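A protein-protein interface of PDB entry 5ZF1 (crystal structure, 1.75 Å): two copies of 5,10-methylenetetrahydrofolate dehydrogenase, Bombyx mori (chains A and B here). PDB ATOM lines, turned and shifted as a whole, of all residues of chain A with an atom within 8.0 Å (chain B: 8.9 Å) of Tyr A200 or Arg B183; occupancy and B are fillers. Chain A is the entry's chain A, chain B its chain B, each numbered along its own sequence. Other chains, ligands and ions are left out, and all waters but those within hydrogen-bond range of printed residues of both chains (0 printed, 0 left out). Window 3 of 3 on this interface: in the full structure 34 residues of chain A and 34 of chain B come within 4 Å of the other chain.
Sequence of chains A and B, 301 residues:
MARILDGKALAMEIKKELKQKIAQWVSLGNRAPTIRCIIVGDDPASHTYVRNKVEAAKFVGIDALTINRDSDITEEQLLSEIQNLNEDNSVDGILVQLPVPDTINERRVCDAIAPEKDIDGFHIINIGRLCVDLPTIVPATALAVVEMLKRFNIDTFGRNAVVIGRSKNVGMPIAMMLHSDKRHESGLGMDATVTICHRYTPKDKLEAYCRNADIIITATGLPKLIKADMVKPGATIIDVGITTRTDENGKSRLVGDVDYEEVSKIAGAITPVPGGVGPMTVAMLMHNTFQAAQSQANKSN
NH1 of Arg A166 is in hydrogen-bond range of O of His B179 (3.1 Å). NH1 of Arg A166 is in salt-bridge range of OD1 of Asp B191 (2.8 Å). A ring nitrogen (NE2) of His A198 lies within hydrogen-bond range of the backbone carbonyl oxygen (O) of Ala B192, 2.9 Å away. The side-chain carboxylate (OD2) of Asp B181 lies within salt-bridge range of the guanidinium group (NH1) of Arg A199 (2.7 Å). OH of Tyr A200 sits at hydrogen-bond distance from NH1 of Arg B183 (3.4 Å). The side-chain hydroxyl of Thr A201 lies within hydrogen-bond range of the side-chain hydroxyl of Thr B193, at 2.9 Å.
A ring nitrogen (ND1) of His A198 sits close to the backbone NH (N) of Tyr A200, 3.1 Å away. The backbone NH (N) of His A198 lies within hydrogen-bond range of the side-chain hydroxyl (OG1) of Thr A201, 3.0 Å away. The side-chain carboxylate (OD2) of Asp B133 is in hydrogen-bond range of the backbone NH (N) of Asp B181. The backbone carbonyl oxygen (O) of Phe B157 lies within hydrogen-bond range of the guanidinium group (NH1) of Arg B159 (2.8 Å). The backbone carbonyl oxygen of Met B190 sits at hydrogen-bond distance from the backbone NH of Phe B157, 3.4 Å away. N of Gly B158 lies within hydrogen-bond range of O of Asp B191 (2.9 Å).
Among the printed residues, pairs that only touch across the chains: Pro A202 with Gly B158 (3.2 Å), Tyr A200 with Asp B191 (3.2 Å), Tyr A200 with Phe B157 (3.3 Å), His A198 with Asp B191 (3.4 Å), Arg A166 with Ser B180 (3.5 Å), Tyr A200 with Gly B158 (3.6 Å), Arg A166 with Asp B181 (3.7 Å), Tyr A200 with Asp B181 (3.7 Å), Lys A205 with Asn B160 (3.8 Å), Cys A197 with Thr B193 (3.9 Å) and Lys A205 with Gly B158 (3.96 Å).
Of the printed residues of chain B, His A198 touches Asp B191 and Ala B192. Printed residues of chain B within 4 Å of Arg A199: Asp B181 (2.7 Å). Tyr A200 touches just these residues of chain B: Phe B157, Gly B158, Asp B181, Arg B183 and Asp B191. Of the printed residues of chain B, Pro A202 touches Gly B158. Of the printed residues of chain A, Gly B158 touches Tyr A200, Pro A202 and Lys A205. No residue of chain A comes within 4 Å of Lys B182. Arg B183 touches just one residue of chain A: Tyr A200. Printed residues of chain A within 4 Å of Ala B192: His A198.
Of the 21 printed residues of chain B, 10 touch a printed residue of chain A. Printed residues of chain B that touch a printed residue of chain A: Phe B157, Gly B158, Asn B160, His B179, Ser B180, Asp B181, Arg B183, Asp B191, Ala B192 and Thr B193. Hydrophobic or aromatic side chains of chain B that line the printed part of chain A: Phe B157. Printed residues of chain A that touch a printed residue of chain B: Arg A166, Cys A197, His A198, Arg A199, Tyr A200, Thr A201, Pro A202 and Lys A205. Hydrophobic or aromatic side chains of chain A within 4 Å of the printed part of chain B: His A198, Tyr A200 and Pro A202. Among the printed residues, 17 pairs touch across the chains. Among the printed residues, Asp or Glu carboxylates within 4 Å of a Lys or Arg side-chain nitrogen of the other chain: Arg A166 with Asp B191 and Arg A199 with Asp B181.
No position is printed for both chains. Of the 17 pairs that touch across the chains among the printed residues, none has its exchanged pair printed and touching as well.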
ATOM      1  N   ARG A 166     -28.837  24.435 -27.281  1.00  0.00           N
ATOM      2  CA  ARG A 166     -27.634  25.186 -26.959  1.00  0.00           C
ATOM      3  C   ARG A 166     -26.570  25.102 -28.037  1.00  0.00           C
ATOM      4  O   ARG A 166     -25.417  25.442 -27.765  1.00  0.00           O
ATOM      5  CB  ARG A 166     -27.001  24.659 -25.669  1.00  0.00           C
ATOM      6  CG  ARG A 166     -27.794  24.774 -24.426  1.00  0.00           C
ATOM      7  CD  ARG A 166     -27.051  24.032 -23.306  1.00  0.00           C
ATOM      8  NE  ARG A 166     -27.128  22.572 -23.420  1.00  0.00           N
ATOM      9  CZ  ARG A 166     -26.787  21.737 -22.438  1.00  0.00           C
ATOM     10  NH1 ARG A 166     -26.331  22.227 -21.287  1.00  0.00           N
ATOM     11  NH2 ARG A 166     -26.891  20.425 -22.589  1.00  0.00           N
ATOM     12  N   CYS A 197     -33.547  26.421 -22.776  1.00  0.00           N
ATOM     13  CA  CYS A 197     -33.876  25.048 -22.395  1.00  0.00           C
ATOM     14  C   CYS A 197     -33.072  24.098 -23.259  1.00  0.00           C
ATOM     15  O   CYS A 197     -32.669  24.442 -24.367  1.00  0.00           O
ATOM     16  CB  CYS A 197     -35.366  24.765 -22.556  1.00  0.00           C
ATOM     17  SG  CYS A 197     -36.420  25.791 -21.505  1.00  0.00           S
ATOM     18  N   HIS A 198     -32.817  22.896 -22.742  1.00  0.00           N
ATOM     19  CA  HIS A 198     -31.919  21.997 -23.460  1.00  0.00           C
ATOM     20  C   HIS A 198     -32.262  20.569 -23.055  1.00  0.00           C
ATOM     21  O   HIS A 198     -33.304  20.319 -22.445  1.00  0.00           O
ATOM     22  CB  HIS A 198     -30.449  22.333 -23.178  1.00  0.00           C
ATOM     23  CG  HIS A 198     -30.128  22.475 -21.721  1.00  0.00           C
ATOM     24  ND1 HIS A 198     -30.082  21.394 -20.864  1.00  0.00           N
ATOM     25  CD2 HIS A 198     -29.842  23.565 -20.972  1.00  0.00           C
ATOM     26  CE1 HIS A 198     -29.776  21.815 -19.646  1.00  0.00           C
ATOM     27  NE2 HIS A 198     -29.613  23.127 -19.686  1.00  0.00           N
ATOM     28  N   ARG A 199     -31.381  19.633 -23.428  1.00  0.00           N
ATOM     29  CA  ARG A 199     -31.727  18.222 -23.317  1.00  0.00           C
ATOM     30  C   ARG A 199     -31.844  17.761 -21.879  1.00  0.00           C
ATOM     31  O   ARG A 199     -32.410  16.690 -21.633  1.00  0.00           O
ATOM     32  CB  ARG A 199     -30.694  17.354 -24.031  1.00  0.00           C
ATOM     33  CG  ARG A 199     -29.336  17.276 -23.377  1.00  0.00           C
ATOM     34  CD  ARG A 199     -28.400  16.434 -24.242  1.00  0.00           C
ATOM     35  NE  ARG A 199     -27.574  17.291 -25.088  1.00  0.00           N
ATOM     36  CZ  ARG A 199     -26.372  17.742 -24.738  1.00  0.00           C
ATOM     37  NH1 ARG A 199     -25.843  17.388 -23.571  1.00  0.00           N
ATOM     38  NH2 ARG A 199     -25.685  18.523 -25.560  1.00  0.00           N
ATOM     39  N   TYR A 200     -31.315  18.509 -20.922  1.00  0.00           N
ATOM     40  CA  TYR A 200     -31.457  18.080 -19.532  1.00  0.00           C
ATOM     41  C   TYR A 200     -32.494  18.895 -18.773  1.00  0.00           C
ATOM     42  O   TYR A 200     -32.662  18.687 -17.569  1.00  0.00           O
ATOM     43  CB  TYR A 200     -30.111  18.132 -18.814  1.00  0.00           C
ATOM     44  CG  TYR A 200     -29.073  17.229 -19.428  1.00  0.00           C
ATOM     45  CD1 TYR A 200     -29.337  15.872 -19.652  1.00  0.00           C
ATOM     46  CD2 TYR A 200     -27.826  17.730 -19.805  1.00  0.00           C
ATOM     47  CE1 TYR A 200     -28.371  15.044 -20.221  1.00  0.00           C
ATOM     48  CE2 TYR A 200     -26.851  16.904 -20.368  1.00  0.00           C
ATOM     49  CZ  TYR A 200     -27.137  15.566 -20.581  1.00  0.00           C
ATOM     50  OH  TYR A 200     -26.187  14.745 -21.145  1.00  0.00           O
ATOM     51  N   THR A 201     -33.178  19.843 -19.426  1.00  0.00           N
ATOM     52  CA  THR A 201     -34.321  20.498 -18.805  1.00  0.00           C
ATOM     53  C   THR A 201     -35.408  19.460 -18.523  1.00  0.00           C
ATOM     54  O   THR A 201     -35.867  18.787 -19.454  1.00  0.00           O
ATOM     55  CB  THR A 201     -34.855  21.643 -19.701  1.00  0.00           C
ATOM     56  OG1 THR A 201     -33.798  22.583 -19.927  1.00  0.00           O
ATOM     57  CG2 THR A 201     -36.012  22.366 -19.042  1.00  0.00           C
ATOM     58  N   PRO A 202     -35.801  19.247 -17.270  1.00  0.00           N
ATOM     59  CA  PRO A 202     -36.836  18.242 -16.996  1.00  0.00           C
ATOM     60  C   PRO A 202     -38.121  18.596 -17.723  1.00  0.00           C
ATOM     61  O   PRO A 202     -38.451  19.774 -17.925  1.00  0.00           O
ATOM     62  CB  PRO A 202     -37.018  18.305 -15.472  1.00  0.00           C
ATOM     63  CG  PRO A 202     -35.776  18.929 -14.958  1.00  0.00           C
ATOM     64  CD  PRO A 202     -35.272  19.865 -16.040  1.00  0.00           C
ATOM     65  N   LYS A 203     -38.856  17.554 -18.113  1.00  0.00           N
ATOM     66  CA  LYS A 203     -39.991  17.754 -19.010  1.00  0.00           C
ATOM     67  C   LYS A 203     -41.005  18.723 -18.427  1.00  0.00           C
ATOM     68  O   LYS A 203     -41.527  19.586 -19.141  1.00  0.00           O
ATOM     69  CB  LYS A 203     -40.668  16.419 -19.317  1.00  0.00           C
ATOM     70  CG  LYS A 203     -41.915  16.552 -20.188  1.00  0.00           C
ATOM     71  CD  LYS A 203     -41.604  17.147 -21.553  1.00  0.00           C
ATOM     72  CE  LYS A 203     -42.843  17.091 -22.448  1.00  0.00           C
ATOM     73  NZ  LYS A 203     -43.560  15.764 -22.314  1.00  0.00           N
ATOM     74  N   LYS A 205     -40.546  21.204 -16.302  1.00  0.00           N
ATOM     75  CA  LYS A 205     -40.082  22.591 -16.336  1.00  0.00           C
ATOM     76  C   LYS A 205     -40.012  23.107 -17.763  1.00  0.00           C
ATOM     77  O   LYS A 205     -40.296  24.289 -18.008  1.00  0.00           O
ATOM     78  CB  LYS A 205     -38.729  22.710 -15.651  1.00  0.00           C
ATOM     79  CG  LYS A 205     -38.857  22.596 -14.155  1.00  0.00           C
ATOM     80  CD  LYS A 205     -37.666  21.951 -13.586  1.00  0.00           C
ATOM     81  CE  LYS A 205     -37.932  21.652 -12.133  1.00  0.00           C
ATOM     82  NZ  LYS A 205     -37.123  20.500 -11.839  1.00  0.00           N
ATOM     83  N   LEU A 206     -39.651  22.249 -18.717  1.00  0.00           N
ATOM     84  CA  LEU A 206     -39.694  22.657 -20.122  1.00  0.00           C
ATOM     85  C   LEU A 206     -41.094  23.119 -20.518  1.00  0.00           C
ATOM     86  O   LEU A 206     -41.265  24.197 -21.109  1.00  0.00           O
ATOM     87  CB  LEU A 206     -39.239  21.508 -21.020  1.00  0.00           C
ATOM     88  CG  LEU A 206     -39.441  21.830 -22.508  1.00  0.00           C
ATOM     89  CD1 LEU A 206     -38.512  22.977 -22.928  1.00  0.00           C
ATOM     90  CD2 LEU A 206     -39.224  20.616 -23.380  1.00  0.00           C
ATOM     91  N   ASP B 133     -18.364  26.768 -25.280  1.00  0.00           N
ATOM     92  CA  ASP B 133     -18.284  25.759 -24.214  1.00  0.00           C
ATOM     93  C   ASP B 133     -17.034  24.881 -24.371  1.00  0.00           C
ATOM     94  O   ASP B 133     -17.092  23.660 -24.244  1.00  0.00           O
ATOM     95  CB  ASP B 133     -19.575  24.921 -24.170  1.00  0.00           C
ATOM     96  CG  ASP B 133     -19.826  24.258 -22.818  1.00  0.00           C
ATOM     97  OD1 ASP B 133     -19.127  24.585 -21.829  1.00  0.00           O
ATOM     98  OD2 ASP B 133     -20.747  23.402 -22.759  1.00  0.00           O
ATOM     99  N   THR B 156     -27.285  22.397  -9.720  1.00  0.00           N
ATOM    100  CA  THR B 156     -27.577  23.155 -10.936  1.00  0.00           C
ATOM    101  C   THR B 156     -28.182  22.304 -12.038  1.00  0.00           C
ATOM    102  O   THR B 156     -28.978  22.804 -12.826  1.00  0.00           O
ATOM    103  CB  THR B 156     -26.292  23.811 -11.473  1.00  0.00           C
ATOM    104  OG1 THR B 156     -25.277  22.814 -11.708  1.00  0.00           O
ATOM    105  CG2 THR B 156     -25.763  24.857 -10.485  1.00  0.00           C
ATOM    106  N   PHE B 157     -27.825  21.015 -12.103  1.00  0.00           N
ATOM    107  CA  PHE B 157     -28.221  20.177 -13.232  1.00  0.00           C
ATOM    108  C   PHE B 157     -29.739  20.061 -13.343  1.00  0.00           C
ATOM    109  O   PHE B 157     -30.393  19.512 -12.449  1.00  0.00           O
ATOM    110  CB  PHE B 157     -27.584  18.786 -13.054  1.00  0.00           C
ATOM    111  CG  PHE B 157     -27.706  17.922 -14.250  1.00  0.00           C
ATOM    112  CD1 PHE B 157     -28.895  17.248 -14.511  1.00  0.00           C
ATOM    113  CD2 PHE B 157     -26.614  17.736 -15.096  1.00  0.00           C
ATOM    114  CE1 PHE B 157     -29.021  16.453 -15.626  1.00  0.00           C
ATOM    115  CE2 PHE B 157     -26.731  16.927 -16.204  1.00  0.00           C
ATOM    116  CZ  PHE B 157     -27.931  16.294 -16.469  1.00  0.00           C
ATOM    117  N   GLY B 158     -30.310  20.596 -14.432  1.00  0.00           N
ATOM    118  CA  GLY B 158     -31.745  20.582 -14.606  1.00  0.00           C
ATOM    119  C   GLY B 158     -32.514  21.518 -13.694  1.00  0.00           C
ATOM    120  O   GLY B 158     -33.742  21.455 -13.682  1.00  0.00           O
ATOM    121  N   ARG B 159     -31.836  22.389 -12.942  1.00  0.00           N
ATOM    122  CA  ARG B 159     -32.533  23.316 -12.060  1.00  0.00           C
ATOM    123  C   ARG B 159     -32.782  24.631 -12.795  1.00  0.00           C
ATOM    124  O   ARG B 159     -32.088  24.958 -13.752  1.00  0.00           O
ATOM    125  CB  ARG B 159     -31.738  23.569 -10.781  1.00  0.00           C
ATOM    126  CG  ARG B 159     -32.049  22.549  -9.628  1.00  0.00           C
ATOM    127  CD  ARG B 159     -31.715  21.131 -10.045  1.00  0.00           C
ATOM    128  NE  ARG B 159     -32.071  20.177  -8.984  1.00  0.00           N
ATOM    129  CZ  ARG B 159     -31.604  18.940  -8.933  1.00  0.00           C
ATOM    130  NH1 ARG B 159     -30.755  18.523  -9.860  1.00  0.00           N
ATOM    131  NH2 ARG B 159     -31.958  18.146  -7.927  1.00  0.00           N
ATOM    132  N   ASN B 160     -33.762  25.382 -12.303  1.00  0.00           N
ATOM    133  CA  ASN B 160     -34.127  26.692 -12.869  1.00  0.00           C
ATOM    134  C   ASN B 160     -33.232  27.772 -12.273  1.00  0.00           C
ATOM    135  O   ASN B 160     -33.289  28.033 -11.065  1.00  0.00           O
ATOM    136  CB  ASN B 160     -35.591  27.008 -12.555  1.00  0.00           C
ATOM    137  CG  ASN B 160     -36.569  26.160 -13.333  1.00  0.00           C
ATOM    138  OD1 ASN B 160     -36.199  25.409 -14.234  1.00  0.00           O
ATOM    139  ND2 ASN B 160     -37.846  26.284 -12.984  1.00  0.00           N
ATOM    140  N   HIS B 179     -25.359  27.271 -17.945  1.00  0.00           N
ATOM    141  CA  HIS B 179     -25.977  26.340 -18.881  1.00  0.00           C
ATOM    142  C   HIS B 179     -24.927  25.577 -19.693  1.00  0.00           C
ATOM    143  O   HIS B 179     -25.236  25.030 -20.748  1.00  0.00           O
ATOM    144  CB  HIS B 179     -27.021  27.042 -19.766  1.00  0.00           C
ATOM    145  CG  HIS B 179     -26.481  28.013 -20.780  1.00  0.00           C
ATOM    146  ND1 HIS B 179     -25.860  27.617 -21.942  1.00  0.00           N
ATOM    147  CD2 HIS B 179     -26.571  29.366 -20.852  1.00  0.00           C
ATOM    148  CE1 HIS B 179     -25.529  28.680 -22.655  1.00  0.00           C
ATOM    149  NE2 HIS B 179     -25.953  29.757 -22.014  1.00  0.00           N
ATOM    150  N   SER B 180     -23.702  25.477 -19.184  1.00  0.00           N
ATOM    151  CA  SER B 180     -22.712  24.699 -19.916  1.00  0.00           C
ATOM    152  C   SER B 180     -23.086  23.225 -19.849  1.00  0.00           C
ATOM    153  O   SER B 180     -23.780  22.790 -18.932  1.00  0.00           O
ATOM    154  CB  SER B 180     -21.305  24.951 -19.373  1.00  0.00           C
ATOM    155  OG  SER B 180     -21.290  25.020 -17.959  1.00  0.00           O
ATOM    156  N   ASP B 181     -22.688  22.473 -20.874  1.00  0.00           N
ATOM    157  CA  ASP B 181     -22.835  21.019 -20.873  1.00  0.00           C
ATOM    158  C   ASP B 181     -21.560  20.424 -20.301  1.00  0.00           C
ATOM    159  O   ASP B 181     -20.469  20.650 -20.834  1.00  0.00           O
ATOM    160  CB  ASP B 181     -23.110  20.474 -22.271  1.00  0.00           C
ATOM    161  CG  ASP B 181     -23.322  18.953 -22.273  1.00  0.00           C
ATOM    162  OD1 ASP B 181     -23.512  18.379 -21.184  1.00  0.00           O
ATOM    163  OD2 ASP B 181     -23.292  18.341 -23.359  1.00  0.00           O
ATOM    164  N   LYS B 182     -21.701  19.671 -19.212  1.00  0.00           N
ATOM    165  CA  LYS B 182     -20.529  19.105 -18.556  1.00  0.00           C
ATOM    166  C   LYS B 182     -19.687  18.287 -19.526  1.00  0.00           C
ATOM    167  O   LYS B 182     -18.453  18.377 -19.510  1.00  0.00           O
ATOM    168  CB  LYS B 182     -20.963  18.259 -17.358  1.00  0.00           C
ATOM    169  N   ARG B 183     -20.340  17.519 -20.407  1.00  0.00           N
ATOM    170  CA  ARG B 183     -19.624  16.573 -21.260  1.00  0.00           C
ATOM    171  C   ARG B 183     -18.626  17.270 -22.172  1.00  0.00           C
ATOM    172  O   ARG B 183     -17.640  16.654 -22.592  1.00  0.00           O
ATOM    173  CB  ARG B 183     -20.608  15.764 -22.108  1.00  0.00           C
ATOM    174  CG  ARG B 183     -21.964  15.562 -21.475  1.00  0.00           C
ATOM    175  CD  ARG B 183     -21.904  14.601 -20.293  1.00  0.00           C
ATOM    176  NE  ARG B 183     -21.586  13.218 -20.658  1.00  0.00           N
ATOM    177  CZ  ARG B 183     -22.354  12.431 -21.412  1.00  0.00           C
ATOM    178  NH1 ARG B 183     -23.496  12.884 -21.919  1.00  0.00           N
ATOM    179  NH2 ARG B 183     -21.978  11.182 -21.663  1.00  0.00           N
ATOM    180  N   HIS B 184     -18.861  18.541 -22.488  1.00  0.00           N
ATOM    181  CA  HIS B 184     -17.996  19.231 -23.430  1.00  0.00           C
ATOM    182  C   HIS B 184     -16.588  19.391 -22.862  1.00  0.00           C
ATOM    183  O   HIS B 184     -16.359  19.320 -21.649  1.00  0.00           O
ATOM    184  CB  HIS B 184     -18.593  20.587 -23.806  1.00  0.00           C
ATOM    185  CG  HIS B 184     -19.782  20.480 -24.707  1.00  0.00           C
ATOM    186  ND1 HIS B 184     -20.410  21.579 -25.253  1.00  0.00           N
ATOM    187  CD2 HIS B 184     -20.456  19.396 -25.161  1.00  0.00           C
ATOM    188  CE1 HIS B 184     -21.422  21.176 -26.003  1.00  0.00           C
ATOM    189  NE2 HIS B 184     -21.471  19.857 -25.964  1.00  0.00           N
ATOM    190  N   GLU B 185     -15.639  19.608 -23.779  1.00  0.00           N
ATOM    191  CA  GLU B 185     -14.223  19.675 -23.425  1.00  0.00           C
ATOM    192  C   GLU B 185     -13.958  20.701 -22.330  1.00  0.00           C
ATOM    193  O   GLU B 185     -13.046  20.522 -21.512  1.00  0.00           O
ATOM    194  CB  GLU B 185     -13.400  20.002 -24.675  1.00  0.00           C
ATOM    195  CG  GLU B 185     -11.906  19.751 -24.551  1.00  0.00           C
ATOM    196  CD  GLU B 185     -11.133  20.231 -25.771  1.00  0.00           C
ATOM    197  OE1 GLU B 185     -11.650  20.095 -26.900  1.00  0.00           O
ATOM    198  OE2 GLU B 185     -10.011  20.747 -25.599  1.00  0.00           O
ATOM    199  N   SER B 186     -14.740  21.788 -22.301  1.00  0.00           N
ATOM    200  CA  SER B 186     -14.561  22.807 -21.269  1.00  0.00           C
ATOM    201  C   SER B 186     -14.664  22.207 -19.873  1.00  0.00           C
ATOM    202  O   SER B 186     -13.857  22.524 -18.988  1.00  0.00           O
ATOM    203  CB  SER B 186     -15.596  23.918 -21.445  1.00  0.00           C
ATOM    204  OG  SER B 186     -15.210  25.099 -20.769  1.00  0.00           O
ATOM    205  N   GLY B 187     -15.644  21.332 -19.658  1.00  0.00           N
ATOM    206  CA  GLY B 187     -15.844  20.721 -18.362  1.00  0.00           C
ATOM    207  C   GLY B 187     -16.454  21.619 -17.308  1.00  0.00           C
ATOM    208  O   GLY B 187     -16.733  21.143 -16.203  1.00  0.00           O
ATOM    209  N   LEU B 188     -16.672  22.893 -17.601  1.00  0.00           N
ATOM    210  CA  LEU B 188     -17.318  23.783 -16.637  1.00  0.00           C
ATOM    211  C   LEU B 188     -18.837  23.680 -16.696  1.00  0.00           C
ATOM    212  O   LEU B 188     -19.554  24.686 -16.626  1.00  0.00           O
ATOM    213  CB  LEU B 188     -16.833  25.210 -16.874  1.00  0.00           C
ATOM    214  CG  LEU B 188     -15.303  25.346 -16.732  1.00  0.00           C
ATOM    215  CD1 LEU B 188     -14.843  26.790 -16.568  1.00  0.00           C
ATOM    216  CD2 LEU B 188     -14.762  24.501 -15.582  1.00  0.00           C
ATOM    217  N   GLY B 189     -19.335  22.444 -16.780  1.00  0.00           N
ATOM    218  CA  GLY B 189     -20.699  22.155 -17.176  1.00  0.00           C
ATOM    219  C   GLY B 189     -21.713  21.993 -16.068  1.00  0.00           C
ATOM    220  O   GLY B 189     -21.794  20.953 -15.407  1.00  0.00           O
ATOM    221  N   MET B 190     -22.547  23.015 -15.918  1.00  0.00           N
ATOM    222  CA  MET B 190     -23.532  23.045 -14.851  1.00  0.00           C
ATOM    223  C   MET B 190     -24.922  22.607 -15.288  1.00  0.00           C
ATOM    224  O   MET B 190     -25.688  22.123 -14.448  1.00  0.00           O
ATOM    225  CB  MET B 190     -23.589  24.454 -14.258  1.00  0.00           C
ATOM    226  CG  MET B 190     -22.227  25.099 -14.220  1.00  0.00           C
ATOM    227  SD  MET B 190     -22.115  26.271 -12.873  1.00  0.00           S
ATOM    228  CE  MET B 190     -21.826  25.196 -11.475  1.00  0.00           C
ATOM    229  N   ASP B 191     -25.274  22.772 -16.566  1.00  0.00           N
ATOM    230  CA  ASP B 191     -26.489  22.173 -17.129  1.00  0.00           C
ATOM    231  C   ASP B 191     -27.765  22.675 -16.453  1.00  0.00           C
ATOM    232  O   ASP B 191     -28.778  21.988 -16.433  1.00  0.00           O
ATOM    233  CB  ASP B 191     -26.417  20.629 -17.067  1.00  0.00           C
ATOM    234  CG  ASP B 191     -25.508  20.050 -18.140  1.00  0.00           C
ATOM    235  OD1 ASP B 191     -25.831  20.247 -19.328  1.00  0.00           O
ATOM    236  OD2 ASP B 191     -24.467  19.409 -17.816  1.00  0.00           O
ATOM    237  N   ALA B 192     -27.754  23.897 -15.939  1.00  0.00           N
ATOM    238  CA  ALA B 192     -28.995  24.502 -15.475  1.00  0.00           C
ATOM    239  C   ALA B 192     -29.818  25.022 -16.655  1.00  0.00           C
ATOM    240  O   ALA B 192     -29.299  25.255 -17.750  1.00  0.00           O
ATOM    241  CB  ALA B 192     -28.707  25.650 -14.509  1.00  0.00           C
ATOM    242  N   THR B 193     -31.115  25.216 -16.405  1.00  0.00           N
ATOM    243  CA  THR B 193     -32.022  25.913 -17.318  1.00  0.00           C
ATOM    244  C   THR B 193     -31.992  27.388 -16.917  1.00  0.00           C
ATOM    245  O   THR B 193     -32.467  27.737 -15.844  1.00  0.00           O
ATOM    246  CB  THR B 193     -33.438  25.352 -17.190  1.00  0.00           C
ATOM    247  OG1 THR B 193     -33.424  23.941 -17.449  1.00  0.00           O
ATOM    248  CG2 THR B 193     -34.391  26.043 -18.189  1.00  0.00           C
